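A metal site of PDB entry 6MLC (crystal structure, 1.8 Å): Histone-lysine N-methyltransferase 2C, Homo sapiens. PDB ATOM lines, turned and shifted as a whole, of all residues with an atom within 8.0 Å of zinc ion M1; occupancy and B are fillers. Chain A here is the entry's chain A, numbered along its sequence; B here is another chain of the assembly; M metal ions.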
ATOM      1  N   TRP A   4       8.058 -22.077  16.483  1.00  0.00           N
ATOM      2  CA  TRP A   4       8.434 -23.311  17.207  1.00  0.00           C
ATOM      3  C   TRP A   4       9.256 -22.939  18.436  1.00  0.00           C
ATOM      4  O   TRP A   4      10.150 -22.089  18.318  1.00  0.00           O
ATOM      5  CB  TRP A   4       9.226 -24.259  16.318  1.00  0.00           C
ATOM      6  CG  TRP A   4       8.345 -24.952  15.342  1.00  0.00           C
ATOM      7  CD1 TRP A   4       7.671 -26.120  15.534  1.00  0.00           C
ATOM      8  CD2 TRP A   4       7.987 -24.464  14.052  1.00  0.00           C
ATOM      9  NE1 TRP A   4       6.942 -26.411  14.417  1.00  0.00           N
ATOM     10  CE2 TRP A   4       7.111 -25.414  13.490  1.00  0.00           C
ATOM     11  CE3 TRP A   4       8.334 -23.336  13.299  1.00  0.00           C
ATOM     12  CZ2 TRP A   4       6.579 -25.270  12.218  1.00  0.00           C
ATOM     13  CZ3 TRP A   4       7.803 -23.195  12.040  1.00  0.00           C
ATOM     14  CH2 TRP A   4       6.930 -24.140  11.509  1.00  0.00           C
ATOM     15  N   CYS A   5       8.984 -23.590  19.555  1.00  0.00           N
ATOM     16  CA  CYS A   5       9.846 -23.539  20.763  1.00  0.00           C
ATOM     17  C   CYS A   5      10.904 -24.644  20.664  1.00  0.00           C
ATOM     18  O   CYS A   5      10.508 -25.820  20.556  1.00  0.00           O
ATOM     19  CB  CYS A   5       9.002 -23.688  21.997  1.00  0.00           C
ATOM     20  SG  CYS A   5       9.998 -23.849  23.502  1.00  0.00           S
ATOM     21  N   ARG A   6      12.201 -24.320  20.754  1.00  0.00           N
ATOM     22  CA  ARG A   6      13.277 -25.333  20.577  1.00  0.00           C
ATOM     23  C   ARG A   6      13.363 -26.181  21.840  1.00  0.00           C
ATOM     24  O   ARG A   6      13.848 -27.321  21.756  1.00  0.00           O
ATOM     25  CB  ARG A   6      14.607 -24.676  20.190  1.00  0.00           C
ATOM     26  CG  ARG A   6      14.568 -23.944  18.857  1.00  0.00           C
ATOM     27  CD  ARG A   6      14.246 -24.845  17.669  1.00  0.00           C
ATOM     28  N   HIS A   7      12.796 -25.723  22.947  1.00  0.00           N
ATOM     29  CA  HIS A   7      12.804 -26.483  24.208  1.00  0.00           C
ATOM     30  C   HIS A   7      11.887 -27.689  24.115  1.00  0.00           C
ATOM     31  O   HIS A   7      12.268 -28.732  24.669  1.00  0.00           O
ATOM     32  CB  HIS A   7      12.390 -25.624  25.408  1.00  0.00           C
ATOM     33  CG  HIS A   7      13.360 -24.564  25.798  1.00  0.00           C
ATOM     34  ND1 HIS A   7      14.624 -24.841  26.366  1.00  0.00           N
ATOM     35  CD2 HIS A   7      13.263 -23.219  25.767  1.00  0.00           C
ATOM     36  CE1 HIS A   7      15.193 -23.728  26.713  1.00  0.00           C
ATOM     37  NE2 HIS A   7      14.390 -22.698  26.356  1.00  0.00           N
ATOM     38  N   CYS A   8      10.641 -27.516  23.591  1.00  0.00           N
ATOM     39  CA  CYS A   8       9.578 -28.567  23.655  1.00  0.00           C
ATOM     40  C   CYS A   8       9.256 -29.094  22.253  1.00  0.00           C
ATOM     41  O   CYS A   8       8.595 -30.156  22.172  1.00  0.00           O
ATOM     42  CB  CYS A   8       8.288 -28.081  24.324  1.00  0.00           C
ATOM     43  SG  CYS A   8       7.514 -26.673  23.488  1.00  0.00           S
ATOM     44  N   GLY A   9       9.627 -28.358  21.196  1.00  0.00           N
ATOM     45  CA  GLY A   9       9.366 -28.749  19.798  1.00  0.00           C
ATOM     46  C   GLY A   9       7.960 -28.386  19.311  1.00  0.00           C
ATOM     47  O   GLY A   9       7.699 -28.559  18.103  1.00  0.00           O
ATOM     48  N   ALA A  10       7.104 -27.825  20.164  1.00  0.00           N
ATOM     49  CA  ALA A  10       5.716 -27.462  19.778  1.00  0.00           C
ATOM     50  C   ALA A  10       5.684 -26.179  18.943  1.00  0.00           C
ATOM     51  O   ALA A  10       6.525 -25.262  19.146  1.00  0.00           O
ATOM     52  CB  ALA A  10       4.850 -27.300  21.001  1.00  0.00           C
ATOM     53  N   THR A  11       4.669 -26.045  18.099  1.00  0.00           N
ATOM     54  CA  THR A  11       4.189 -24.717  17.655  1.00  0.00           C
ATOM     55  C   THR A  11       3.600 -24.024  18.899  1.00  0.00           C
ATOM     56  O   THR A  11       2.965 -24.708  19.739  1.00  0.00           O
ATOM     57  CB  THR A  11       3.207 -24.779  16.486  1.00  0.00           C
ATOM     58  OG1 THR A  11       1.965 -25.268  16.994  1.00  0.00           O
ATOM     59  CG2 THR A  11       3.766 -25.576  15.318  1.00  0.00           C
ATOM     60  N   SER A  12       3.912 -22.767  19.068  1.00  0.00           N
ATOM     61  CA  SER A  12       3.846 -22.080  20.376  1.00  0.00           C
ATOM     62  C   SER A  12       3.399 -20.623  20.214  1.00  0.00           C
ATOM     63  O   SER A  12       3.763 -20.036  19.220  1.00  0.00           O
ATOM     64  CB  SER A  12       5.191 -22.157  21.060  1.00  0.00           C
ATOM     65  OG  SER A  12       5.118 -21.553  22.324  1.00  0.00           O
ATOM     66  N   GLY A  14       4.745 -18.617  22.211  1.00  0.00           N
ATOM     67  CA  GLY A  14       6.022 -18.025  22.652  1.00  0.00           C
ATOM     68  C   GLY A  14       5.800 -17.089  23.821  1.00  0.00           C
ATOM     69  O   GLY A  14       6.211 -15.914  23.752  1.00  0.00           O
ATOM     70  N   LEU A  15       5.109 -17.583  24.853  1.00  0.00           N
ATOM     71  CA  LEU A  15       4.826 -16.818  26.096  1.00  0.00           C
ATOM     72  C   LEU A  15       6.139 -16.614  26.835  1.00  0.00           C
ATOM     73  O   LEU A  15       7.109 -17.365  26.607  1.00  0.00           O
ATOM     74  CB  LEU A  15       3.829 -17.558  26.973  1.00  0.00           C
ATOM     75  CG  LEU A  15       2.481 -17.837  26.318  1.00  0.00           C
ATOM     76  CD1 LEU A  15       1.534 -18.450  27.301  1.00  0.00           C
ATOM     77  CD2 LEU A  15       1.899 -16.563  25.725  1.00  0.00           C
ATOM     78  N   CYS A  29      16.119 -18.376  28.137  1.00  0.00           N
ATOM     79  CA  CYS A  29      14.935 -17.705  27.539  1.00  0.00           C
ATOM     80  C   CYS A  29      15.067 -16.183  27.611  1.00  0.00           C
ATOM     81  O   CYS A  29      14.855 -15.562  26.593  1.00  0.00           O
ATOM     82  CB  CYS A  29      13.626 -18.163  28.168  1.00  0.00           C
ATOM     83  SG  CYS A  29      13.231 -19.866  27.721  1.00  0.00           S
ATOM     84  N   VAL B   3       2.871 -32.697  27.537  1.00  0.00           N
ATOM     85  CA  VAL B   3       3.635 -32.033  28.621  1.00  0.00           C
ATOM     86  C   VAL B   3       3.454 -30.516  28.471  1.00  0.00           C
ATOM     87  O   VAL B   3       3.453 -30.030  27.319  1.00  0.00           O
ATOM     88  CB  VAL B   3       5.122 -32.441  28.573  1.00  0.00           C
ATOM     89  CG1 VAL B   3       5.855 -31.804  27.415  1.00  0.00           C
ATOM     90  CG2 VAL B   3       5.828 -32.137  29.884  1.00  0.00           C
ATOM     91  N   TRP B   4       3.373 -29.813  29.585  1.00  0.00           N
ATOM     92  CA  TRP B   4       3.406 -28.336  29.643  1.00  0.00           C
ATOM     93  C   TRP B   4       4.856 -27.856  29.570  1.00  0.00           C
ATOM     94  O   TRP B   4       5.670 -28.236  30.416  1.00  0.00           O
ATOM     95  CB  TRP B   4       2.728 -27.832  30.905  1.00  0.00           C
ATOM     96  CG  TRP B   4       2.875 -26.357  31.119  1.00  0.00           C
ATOM     97  CD1 TRP B   4       2.808 -25.366  30.178  1.00  0.00           C
ATOM     98  CD2 TRP B   4       3.053 -25.700  32.378  1.00  0.00           C
ATOM     99  NE1 TRP B   4       2.928 -24.140  30.772  1.00  0.00           N
ATOM    100  CE2 TRP B   4       3.106 -24.316  32.124  1.00  0.00           C
ATOM    101  CE3 TRP B   4       3.214 -26.158  33.685  1.00  0.00           C
ATOM    102  CZ2 TRP B   4       3.277 -23.382  33.144  1.00  0.00           C
ATOM    103  CZ3 TRP B   4       3.351 -25.237  34.695  1.00  0.00           C
ATOM    104  CH2 TRP B   4       3.401 -23.863  34.424  1.00  0.00           C
ATOM    105  N   CYS B   5       5.149 -27.017  28.596  1.00  0.00           N
ATOM    106  CA  CYS B   5       6.446 -26.335  28.504  1.00  0.00           C
ATOM    107  C   CYS B   5       6.372 -25.002  29.245  1.00  0.00           C
ATOM    108  O   CYS B   5       5.734 -24.070  28.752  1.00  0.00           O
ATOM    109  CB  CYS B   5       6.839 -26.097  27.064  1.00  0.00           C
ATOM    110  SG  CYS B   5       8.473 -25.342  26.976  1.00  0.00           S
ATOM    111  N   ARG B   6       7.070 -24.909  30.376  1.00  0.00           N
ATOM    112  CA  ARG B   6       7.098 -23.685  31.208  1.00  0.00           C
ATOM    113  C   ARG B   6       7.838 -22.575  30.455  1.00  0.00           C
ATOM    114  O   ARG B   6       7.595 -21.430  30.751  1.00  0.00           O
ATOM    115  CB  ARG B   6       7.755 -23.983  32.558  1.00  0.00           C
ATOM    116  CG  ARG B   6       6.796 -24.560  33.580  1.00  0.00           C
ATOM    117  CD  ARG B   6       7.523 -24.657  34.908  1.00  0.00           C
ATOM    118  NE  ARG B   6       6.647 -24.580  36.065  1.00  0.00           N
ATOM    119  CZ  ARG B   6       5.992 -25.605  36.580  1.00  0.00           C
ATOM    120  NH1 ARG B   6       5.247 -25.435  37.661  1.00  0.00           N
ATOM    121  NH2 ARG B   6       6.053 -26.797  36.016  1.00  0.00           N
ATOM    122  N   HIS B   7       8.728 -22.934  29.516  1.00  0.00           N
ATOM    123  CA  HIS B   7       9.524 -21.967  28.730  1.00  0.00           C
ATOM    124  C   HIS B   7       8.663 -21.124  27.791  1.00  0.00           C
ATOM    125  O   HIS B   7       9.039 -19.947  27.540  1.00  0.00           O
ATOM    126  CB  HIS B   7      10.626 -22.674  27.929  1.00  0.00           C
ATOM    127  CG  HIS B   7      11.634 -23.421  28.741  1.00  0.00           C
ATOM    128  ND1 HIS B   7      12.670 -22.769  29.458  1.00  0.00           N
ATOM    129  CD2 HIS B   7      11.852 -24.751  28.859  1.00  0.00           C
ATOM    130  CE1 HIS B   7      13.419 -23.672  30.020  1.00  0.00           C
ATOM    131  NE2 HIS B   7      12.940 -24.917  29.663  1.00  0.00           N
ATOM    132  N   CYS B   8       7.645 -21.701  27.144  1.00  0.00           N
ATOM    133  CA  CYS B   8       6.877 -21.023  26.062  1.00  0.00           C
ATOM    134  C   CYS B   8       5.370 -21.059  26.321  1.00  0.00           C
ATOM    135  O   CYS B   8       4.644 -20.340  25.651  1.00  0.00           O
ATOM    136  CB  CYS B   8       7.216 -21.636  24.711  1.00  0.00           C
ATOM    137  SG  CYS B   8       6.415 -23.227  24.421  1.00  0.00           S
ATOM    138  N   GLY B   9       4.922 -21.888  27.247  1.00  0.00           N
ATOM    139  CA  GLY B   9       3.507 -21.984  27.618  1.00  0.00           C
ATOM    140  C   GLY B   9       2.764 -23.062  26.826  1.00  0.00           C
ATOM    141  O   GLY B   9       1.646 -23.385  27.183  1.00  0.00           O
ATOM    142  N   ALA B  10       3.368 -23.630  25.776  1.00  0.00           N
ATOM    143  CA  ALA B  10       2.688 -24.571  24.872  1.00  0.00           C
ATOM    144  C   ALA B  10       2.473 -25.888  25.605  1.00  0.00           C
ATOM    145  O   ALA B  10       3.298 -26.264  26.458  1.00  0.00           O
ATOM    146  CB  ALA B  10       3.474 -24.766  23.599  1.00  0.00           C
ATOM    147  N   THR B  11       1.424 -26.609  25.222  1.00  0.00           N
ATOM    148  CA  THR B  11       1.322 -28.069  25.400  1.00  0.00           C
ATOM    149  C   THR B  11       2.011 -28.741  24.208  1.00  0.00           C
ATOM    150  O   THR B  11       1.757 -28.305  23.047  1.00  0.00           O
ATOM    151  CB  THR B  11      -0.135 -28.522  25.575  1.00  0.00           C
ATOM    152  OG1 THR B  11      -0.674 -27.827  26.692  1.00  0.00           O
ATOM    153  CG2 THR B  11      -0.259 -30.019  25.801  1.00  0.00           C
ATOM    154  N   SER B  12       2.818 -29.764  24.479  1.00  0.00           N
ATOM    155  CA  SER B  12       3.681 -30.471  23.498  1.00  0.00           C
ATOM    156  C   SER B  12       3.542 -31.986  23.692  1.00  0.00           C
ATOM    157  O   SER B  12       3.181 -32.441  24.831  1.00  0.00           O
ATOM    158  CB  SER B  12       5.121 -30.031  23.614  1.00  0.00           C
ATOM    159  OG  SER B  12       5.952 -30.719  22.698  1.00  0.00           O
ATOM    160  N   CYS B  29      16.632 -28.051  30.828  1.00  0.00           N
ATOM    161  CA  CYS B  29      15.728 -29.135  30.312  1.00  0.00           C
ATOM    162  C   CYS B  29      16.304 -30.516  30.665  1.00  0.00           C
ATOM    163  O   CYS B  29      15.550 -31.331  31.182  1.00  0.00           O
ATOM    164  CB  CYS B  29      15.469 -29.011  28.817  1.00  0.00           C
ATOM    165  SG  CYS B  29      14.295 -27.682  28.447  1.00  0.00           S
HETATM  166 ZN    ZN M   1       8.196 -24.833  24.670  1.00  0.00          ZN
HETATM  167 ZN    ZN M   2      15.618 -26.551  26.986  1.00  0.00          ZN
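Zinc ion M1 is bound by SG of Cys 8 of chain A (2.3 Å), SG of Cys 5 of chain A (2.4 Å), SG of Cys 5 of chain B (2.4 Å) and SG of Cys 8 of chain B (2.4 Å). Zinc ion M1 has four donor atoms within binding distance.
The nearest printed residue that does not touch zinc ion M1 is His 7 of chain A (4.3 Å).
N of Ala 10 of chain A lies close to SG of Cys 8 of chain A (3.5 Å). OG of Ser 12 of chain B lies within hydrogen-bond range of O of Cys 8 of chain A (2.8 Å). O of Ala 10 of chain A lies within hydrogen-bond range of N of Cys 5 of chain A (3.0 Å). The side-chain sulfur of Cys 5 of chain B sits close to the backbone NH of His 7 of chain B. The backbone carbonyl oxygen (O) of Ala 10 of chain B lies within hydrogen-bond range of the backbone NH (N) of Cys 5 of chain B, at 2.9 Å. SG of Cys 8 of chain B lies close to N of Ala 10 of chain B, 3.4 Å away. The side-chain sulfur (SG) of Cys 8 of chain B sits close to the side-chain hydroxyl (OG) of Ser 12 of chain A, at 3.0 Å. O of Cys 8 of chain B lies within hydrogen-bond range of N of Leu 15 (2.9 Å).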
